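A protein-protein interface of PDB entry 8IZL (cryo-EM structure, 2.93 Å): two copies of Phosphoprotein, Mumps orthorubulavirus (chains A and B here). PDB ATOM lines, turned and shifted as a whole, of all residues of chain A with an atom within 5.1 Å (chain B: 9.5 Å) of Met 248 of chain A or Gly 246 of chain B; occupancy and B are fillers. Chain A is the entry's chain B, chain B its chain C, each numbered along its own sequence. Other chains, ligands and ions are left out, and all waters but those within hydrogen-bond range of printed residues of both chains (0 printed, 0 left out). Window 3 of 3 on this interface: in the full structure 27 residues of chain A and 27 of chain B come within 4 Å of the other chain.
The side-chain sulfur (SD) of Met 248 of chain A lies within hydrogen-bond range of the backbone NH (N) of Thr 250 of chain B, at 3.1 Å. SD of Met 248 of chain A sits close to O of Gly 246 of chain B, 3.3 Å away. N of Gly 246 of chain B sits at hydrogen-bond distance from OE1 of Gln 245 of chain A (3.4 Å). The side-chain amide oxygen (OE1) of Gln 251 of chain A lies close to the side-chain amino group (NZ) of Lys 253 of chain B (3.3 Å). The backbone carbonyl oxygen (O) of Val 249 of chain B lies close to the side-chain sulfur (SD) of Met 248 of chain A (3.1 Å).
Of the 16 printed residues of chain B, 5 touch a printed residue of chain A. Hydrophobic or aromatic side chains of chain B that line the printed part of chain A: Val 249. Hydrophobic or aromatic side chains of chain A within 4 Å of the printed part of chain B: Met 248 and Ile 252. Among the printed residues, no Asp or Glu carboxylate lies within 4 Å of a Lys or Arg side-chain nitrogen of the other chain.
No residue of chain B comes within 4 Å of Gly 246 of chain A. No residue of chain B comes within 4 Å of Ser 247 of chain A. Of chain B, only Gly 246, Val 249 and Thr 250 come within 4 Å of Met 248 of chain A. No residue of chain B comes within 4 Å of Val 249 of chain A. Of the printed residues of chain B, Gln 251 of chain A touches Lys 253. Of the printed residues of chain B, Ile 252 of chain A touches Lys 253. Of the printed residues of chain A, Leu 243 of chain B touches Gln 245 (3.7 Å). Of chain A, only Gln 245 (3.4 Å) and Met 248 (3.1 Å) come within 4 Å of Gly 246 of chain B. Of the printed residues of chain A, Val 249 of chain B touches Met 248 (3.1 Å). Of the printed residues of chain A, Lys 253 of chain B touches Gln 251 and Ile 252. The nearest residue of chain B that does not touch Met 248 of chain A is Lys 253 of chain B (4.1 Å). The nearest printed residue of chain A that does not touch Gly 246 of chain B is Gly 246 of chain A (6.7 Å). The nearest printed residue of chain B that does not touch Ile 252 of chain A is Leu 256 of chain B (4.1 Å).
Gln 245 of chain A touches Gly 246 of chain B, but with the chains exchanged Gly 246 of chain A does not touch Gln 245 of chain B (8.5 Å). Met 248 of chain A touches Gly 246 of chain B, but with the chains exchanged Gly 246 of chain A does not touch Met 248 of chain B (11.0 Å). Met 248 of chain A touches Val 249 of chain B, but with the chains exchanged Val 249 of chain A does not touch Met 248 of chain B (9.1 Å). Met 248 of chain A touches Thr 250 of chain B, but with the chains exchanged Thr 250 of chain A does not touch Met 248 of chain B (12.3 Å). 8 positions are printed for both chains. Of the 7 pairs that touch across the chains among the printed residues, none has its exchanged pair printed and touching as well.
O of Thr 250 of chain B lies close to OD1 of Asn 254 of chain B (2.8 Å).
Among the printed residues, pairs that only touch across the chains: Gln 245 of chain A with Leu 243 of chain B (3.7 Å) and Ile 252 of chain A with Lys 253 of chain B (3.7 Å).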
ATOM      1  N   GLN A 245      16.503  24.442 -15.260  1.00  0.00           N
ATOM      2  CA  GLN A 245      17.015  23.332 -16.111  1.00  0.00           C
ATOM      3  C   GLN A 245      17.322  22.103 -15.249  1.00  0.00           C
ATOM      4  O   GLN A 245      17.578  21.029 -15.830  1.00  0.00           O
ATOM      5  CB  GLN A 245      18.261  23.772 -16.880  1.00  0.00           C
ATOM      6  CG  GLN A 245      17.978  24.790 -17.977  1.00  0.00           C
ATOM      7  CD  GLN A 245      19.243  25.286 -18.632  1.00  0.00           C
ATOM      8  OE1 GLN A 245      20.347  24.856 -18.305  1.00  0.00           O
ATOM      9  NE2 GLN A 245      19.090  26.206 -19.571  1.00  0.00           N
ATOM     10  N   GLY A 246      17.240  22.254 -13.925  1.00  0.00           N
ATOM     11  CA  GLY A 246      17.646  21.167 -13.010  1.00  0.00           C
ATOM     12  C   GLY A 246      16.617  20.073 -12.815  1.00  0.00           C
ATOM     13  O   GLY A 246      17.030  18.929 -12.595  1.00  0.00           O
ATOM     14  N   SER A 247      15.324  20.386 -12.860  1.00  0.00           N
ATOM     15  CA  SER A 247      14.350  19.308 -12.561  1.00  0.00           C
ATOM     16  C   SER A 247      14.724  18.092 -13.402  1.00  0.00           C
ATOM     17  O   SER A 247      14.809  16.982 -12.848  1.00  0.00           O
ATOM     18  CB  SER A 247      12.954  19.752 -12.849  1.00  0.00           C
ATOM     19  OG  SER A 247      12.632  20.909 -12.094  1.00  0.00           O
ATOM     20  N   MET A 248      14.957  18.317 -14.696  1.00  0.00           N
ATOM     21  CA  MET A 248      15.363  17.212 -15.592  1.00  0.00           C
ATOM     22  C   MET A 248      16.345  16.339 -14.818  1.00  0.00           C
ATOM     23  O   MET A 248      16.165  15.109 -14.813  1.00  0.00           O
ATOM     24  CB  MET A 248      16.041  17.775 -16.836  1.00  0.00           C
ATOM     25  CG  MET A 248      16.704  16.736 -17.683  1.00  0.00           C
ATOM     26  SD  MET A 248      17.515  17.652 -18.987  1.00  0.00           S
ATOM     27  CE  MET A 248      18.048  19.091 -18.063  1.00  0.00           C
ATOM     28  N   VAL A 249      17.308  16.970 -14.149  1.00  0.00           N
ATOM     29  CA  VAL A 249      18.330  16.185 -13.426  1.00  0.00           C
ATOM     30  C   VAL A 249      17.563  15.295 -12.464  1.00  0.00           C
ATOM     31  O   VAL A 249      17.622  14.078 -12.603  1.00  0.00           O
ATOM     32  CB  VAL A 249      19.333  17.097 -12.703  1.00  0.00           C
ATOM     33  CG1 VAL A 249      20.254  16.317 -11.780  1.00  0.00           C
ATOM     34  CG2 VAL A 249      20.141  17.917 -13.692  1.00  0.00           C
ATOM     35  N   THR A 250      16.813  15.887 -11.553  1.00  0.00           N
ATOM     36  CA  THR A 250      16.190  15.000 -10.550  1.00  0.00           C
ATOM     37  C   THR A 250      15.633  13.769 -11.247  1.00  0.00           C
ATOM     38  O   THR A 250      16.137  12.667 -10.984  1.00  0.00           O
ATOM     39  CB  THR A 250      15.071  15.707  -9.795  1.00  0.00           C
ATOM     40  OG1 THR A 250      14.018  15.947 -10.728  1.00  0.00           O
ATOM     41  CG2 THR A 250      15.516  17.012  -9.177  1.00  0.00           C
ATOM     42  N   GLN A 251      14.629  13.944 -12.098  1.00  0.00           N
ATOM     43  CA  GLN A 251      13.996  12.735 -12.674  1.00  0.00           C
ATOM     44  C   GLN A 251      15.112  11.809 -13.098  1.00  0.00           C
ATOM     45  O   GLN A 251      15.000  10.598 -12.900  1.00  0.00           O
ATOM     46  CB  GLN A 251      13.183  13.024 -13.926  1.00  0.00           C
ATOM     47  CG  GLN A 251      12.600  11.762 -14.542  1.00  0.00           C
ATOM     48  CD  GLN A 251      12.059  11.998 -15.927  1.00  0.00           C
ATOM     49  OE1 GLN A 251      12.056  13.119 -16.429  1.00  0.00           O
ATOM     50  NE2 GLN A 251      11.596  10.931 -16.559  1.00  0.00           N
ATOM     51  N   ILE A 252      16.165  12.390 -13.639  1.00  0.00           N
ATOM     52  CA  ILE A 252      17.168  11.464 -14.154  1.00  0.00           C
ATOM     53  C   ILE A 252      17.820  10.692 -13.015  1.00  0.00           C
ATOM     54  O   ILE A 252      18.160   9.517 -13.179  1.00  0.00           O
ATOM     55  CB  ILE A 252      18.201  12.202 -15.034  1.00  0.00           C
ATOM     56  CG1 ILE A 252      18.703  11.280 -16.145  1.00  0.00           C
ATOM     57  CG2 ILE A 252      19.386  12.704 -14.222  1.00  0.00           C
ATOM     58  CD1 ILE A 252      17.661  10.966 -17.193  1.00  0.00           C
ATOM     59  N   VAL B 239      26.817  32.750 -19.598  1.00  0.00           N
ATOM     60  CA  VAL B 239      25.503  32.109 -19.636  1.00  0.00           C
ATOM     61  C   VAL B 239      25.164  31.677 -21.060  1.00  0.00           C
ATOM     62  O   VAL B 239      24.525  30.633 -21.266  1.00  0.00           O
ATOM     63  CB  VAL B 239      24.413  33.020 -19.037  1.00  0.00           C
ATOM     64  CG1 VAL B 239      24.522  34.422 -19.571  1.00  0.00           C
ATOM     65  CG2 VAL B 239      23.030  32.447 -19.295  1.00  0.00           C
ATOM     66  N   LYS B 241      27.213  30.456 -23.016  1.00  0.00           N
ATOM     67  CA  LYS B 241      27.961  29.182 -23.200  1.00  0.00           C
ATOM     68  C   LYS B 241      27.277  28.056 -22.418  1.00  0.00           C
ATOM     69  O   LYS B 241      27.327  26.903 -22.891  1.00  0.00           O
ATOM     70  CB  LYS B 241      29.413  29.369 -22.745  1.00  0.00           C
ATOM     71  CG  LYS B 241      29.997  28.225 -21.929  1.00  0.00           C
ATOM     72  CD  LYS B 241      31.379  28.519 -21.385  1.00  0.00           C
ATOM     73  CE  LYS B 241      31.941  27.381 -20.558  1.00  0.00           C
ATOM     74  NZ  LYS B 241      33.314  27.674 -20.087  1.00  0.00           N
ATOM     75  N   VAL B 242      26.641  28.367 -21.285  1.00  0.00           N
ATOM     76  CA  VAL B 242      26.073  27.273 -20.435  1.00  0.00           C
ATOM     77  C   VAL B 242      24.612  26.987 -20.811  1.00  0.00           C
ATOM     78  O   VAL B 242      24.055  26.021 -20.254  1.00  0.00           O
ATOM     79  CB  VAL B 242      26.212  27.594 -18.933  1.00  0.00           C
ATOM     80  CG1 VAL B 242      27.659  27.849 -18.543  1.00  0.00           C
ATOM     81  CG2 VAL B 242      25.326  28.755 -18.514  1.00  0.00           C
ATOM     82  N   LEU B 243      24.008  27.774 -21.709  1.00  0.00           N
ATOM     83  CA  LEU B 243      22.593  27.542 -21.996  1.00  0.00           C
ATOM     84  C   LEU B 243      22.320  26.189 -22.651  1.00  0.00           C
ATOM     85  O   LEU B 243      21.190  25.696 -22.569  1.00  0.00           O
ATOM     86  CB  LEU B 243      22.035  28.672 -22.872  1.00  0.00           C
ATOM     87  CG  LEU B 243      22.654  29.061 -24.221  1.00  0.00           C
ATOM     88  CD1 LEU B 243      22.363  28.055 -25.333  1.00  0.00           C
ATOM     89  CD2 LEU B 243      22.200  30.457 -24.632  1.00  0.00           C
ATOM     90  N   ALA B 244      23.313  25.577 -23.297  1.00  0.00           N
ATOM     91  CA  ALA B 244      23.094  24.301 -23.973  1.00  0.00           C
ATOM     92  C   ALA B 244      23.211  23.103 -23.039  1.00  0.00           C
ATOM     93  O   ALA B 244      22.869  21.980 -23.442  1.00  0.00           O
ATOM     94  CB  ALA B 244      24.080  24.146 -25.133  1.00  0.00           C
ATOM     95  N   GLN B 245      23.700  23.312 -21.814  1.00  0.00           N
ATOM     96  CA  GLN B 245      23.896  22.197 -20.895  1.00  0.00           C
ATOM     97  C   GLN B 245      22.573  21.539 -20.528  1.00  0.00           C
ATOM     98  O   GLN B 245      22.473  20.308 -20.509  1.00  0.00           O
ATOM     99  CB  GLN B 245      24.636  22.672 -19.645  1.00  0.00           C
ATOM    100  CG  GLN B 245      26.096  23.025 -19.893  1.00  0.00           C
ATOM    101  CD  GLN B 245      26.854  23.332 -18.614  1.00  0.00           C
ATOM    102  OE1 GLN B 245      26.256  23.541 -17.559  1.00  0.00           O
ATOM    103  NE2 GLN B 245      28.179  23.349 -18.702  1.00  0.00           N
ATOM    104  N   GLY B 246      21.542  22.336 -20.249  1.00  0.00           N
ATOM    105  CA  GLY B 246      20.246  21.761 -19.920  1.00  0.00           C
ATOM    106  C   GLY B 246      19.631  20.996 -21.077  1.00  0.00           C
ATOM    107  O   GLY B 246      18.995  19.956 -20.882  1.00  0.00           O
ATOM    108  N   SER B 247      20.005  21.395 -22.296  1.00  0.00           N
ATOM    109  CA  SER B 247      19.531  20.661 -23.496  1.00  0.00           C
ATOM    110  C   SER B 247      20.369  19.398 -23.684  1.00  0.00           C
ATOM    111  O   SER B 247      19.789  18.339 -23.949  1.00  0.00           O
ATOM    112  CB  SER B 247      19.602  21.520 -24.720  1.00  0.00           C
ATOM    113  OG  SER B 247      20.950  21.710 -25.120  1.00  0.00           O
ATOM    114  N   MET B 248      21.691  19.508 -23.593  1.00  0.00           N
ATOM    115  CA  MET B 248      22.483  18.258 -23.668  1.00  0.00           C
ATOM    116  C   MET B 248      21.875  17.324 -22.628  1.00  0.00           C
ATOM    117  O   MET B 248      21.489  16.196 -22.984  1.00  0.00           O
ATOM    118  CB  MET B 248      23.950  18.517 -23.324  1.00  0.00           C
ATOM    119  CG  MET B 248      24.898  17.544 -23.985  1.00  0.00           C
ATOM    120  SD  MET B 248      26.172  16.977 -22.840  1.00  0.00           S
ATOM    121  CE  MET B 248      25.155  16.109 -21.647  1.00  0.00           C
ATOM    122  N   VAL B 249      21.753  17.812 -21.392  1.00  0.00           N
ATOM    123  CA  VAL B 249      21.218  16.956 -20.302  1.00  0.00           C
ATOM    124  C   VAL B 249      19.819  16.537 -20.724  1.00  0.00           C
ATOM    125  O   VAL B 249      19.350  15.483 -20.279  1.00  0.00           O
ATOM    126  CB  VAL B 249      21.250  17.662 -18.938  1.00  0.00           C
ATOM    127  CG1 VAL B 249      20.652  16.792 -17.846  1.00  0.00           C
ATOM    128  CG2 VAL B 249      22.668  18.047 -18.555  1.00  0.00           C
ATOM    129  N   THR B 250      19.181  17.312 -21.589  1.00  0.00           N
ATOM    130  CA  THR B 250      17.878  16.774 -22.034  1.00  0.00           C
ATOM    131  C   THR B 250      18.117  15.728 -23.117  1.00  0.00           C
ATOM    132  O   THR B 250      17.398  14.720 -23.091  1.00  0.00           O
ATOM    133  CB  THR B 250      16.890  17.874 -22.422  1.00  0.00           C
ATOM    134  OG1 THR B 250      15.619  17.444 -21.935  1.00  0.00           O
ATOM    135  CG2 THR B 250      16.816  18.125 -23.911  1.00  0.00           C
ATOM    136  N   GLN B 251      19.071  15.947 -24.042  1.00  0.00           N
ATOM    137  CA  GLN B 251      19.249  14.834 -24.970  1.00  0.00           C
ATOM    138  C   GLN B 251      19.517  13.531 -24.227  1.00  0.00           C
ATOM    139  O   GLN B 251      18.947  12.486 -24.560  1.00  0.00           O
ATOM    140  CB  GLN B 251      20.384  15.132 -25.949  1.00  0.00           C
ATOM    141  CG  GLN B 251      20.078  16.236 -26.947  1.00  0.00           C
ATOM    142  CD  GLN B 251      21.293  16.620 -27.769  1.00  0.00           C
ATOM    143  OE1 GLN B 251      22.315  15.935 -27.745  1.00  0.00           O
ATOM    144  NE2 GLN B 251      21.186  17.724 -28.502  1.00  0.00           N
ATOM    145  N   ILE B 252      20.388  13.569 -23.215  1.00  0.00           N
ATOM    146  CA  ILE B 252      20.696  12.354 -22.466  1.00  0.00           C
ATOM    147  C   ILE B 252      19.496  11.873 -21.663  1.00  0.00           C
ATOM    148  O   ILE B 252      19.440  10.698 -21.285  1.00  0.00           O
ATOM    149  CB  ILE B 252      21.922  12.568 -21.556  1.00  0.00           C
ATOM    150  CG1 ILE B 252      21.601  13.511 -20.391  1.00  0.00           C
ATOM    151  CG2 ILE B 252      23.093  13.106 -22.360  1.00  0.00           C
ATOM    152  CD1 ILE B 252      21.310  12.810 -19.073  1.00  0.00           C
ATOM    153  N   LYS B 253      18.531  12.755 -21.386  1.00  0.00           N
ATOM    154  CA  LYS B 253      17.348  12.345 -20.639  1.00  0.00           C
ATOM    155  C   LYS B 253      16.519  11.333 -21.421  1.00  0.00           C
ATOM    156  O   LYS B 253      16.073  10.324 -20.862  1.00  0.00           O
ATOM    157  CB  LYS B 253      16.509  13.571 -20.276  1.00  0.00           C
ATOM    158  CG  LYS B 253      15.007  13.321 -20.237  1.00  0.00           C
ATOM    159  CD  LYS B 253      14.587  12.652 -18.939  1.00  0.00           C
ATOM    160  CE  LYS B 253      13.229  11.989 -19.087  1.00  0.00           C
ATOM    161  NZ  LYS B 253      12.230  12.915 -19.686  1.00  0.00           N
ATOM    162  N   ASN B 254      16.301  11.581 -22.715  1.00  0.00           N
ATOM    163  CA  ASN B 254      15.502  10.652 -23.509  1.00  0.00           C
ATOM    164  C   ASN B 254      16.286   9.388 -23.839  1.00  0.00           C
ATOM    165  O   ASN B 254      15.728   8.286 -23.823  1.00  0.00           O
ATOM    166  CB  ASN B 254      15.010  11.335 -24.788  1.00  0.00           C
ATOM    167  CG  ASN B 254      16.100  12.120 -25.486  1.00  0.00           C
ATOM    168  OD1 ASN B 254      16.276  13.315 -25.239  1.00  0.00           O
ATOM    169  ND2 ASN B 254      16.837  11.457 -26.369  1.00  0.00           N
ATOM    170  N   LEU B 256      18.667   7.948 -22.096  1.00  0.00           N
ATOM    171  CA  LEU B 256      18.770   7.093 -20.920  1.00  0.00           C
ATOM    172  C   LEU B 256      17.478   6.317 -20.699  1.00  0.00           C
ATOM    173  O   LEU B 256      17.513   5.173 -20.227  1.00  0.00           O
ATOM    174  CB  LEU B 256      19.139   7.946 -19.700  1.00  0.00           C
ATOM    175  CG  LEU B 256      19.458   7.395 -18.300  1.00  0.00           C
ATOM    176  CD1 LEU B 256      18.277   6.756 -17.582  1.00  0.00           C
ATOM    177  CD2 LEU B 256      20.619   6.416 -18.388  1.00  0.00           C
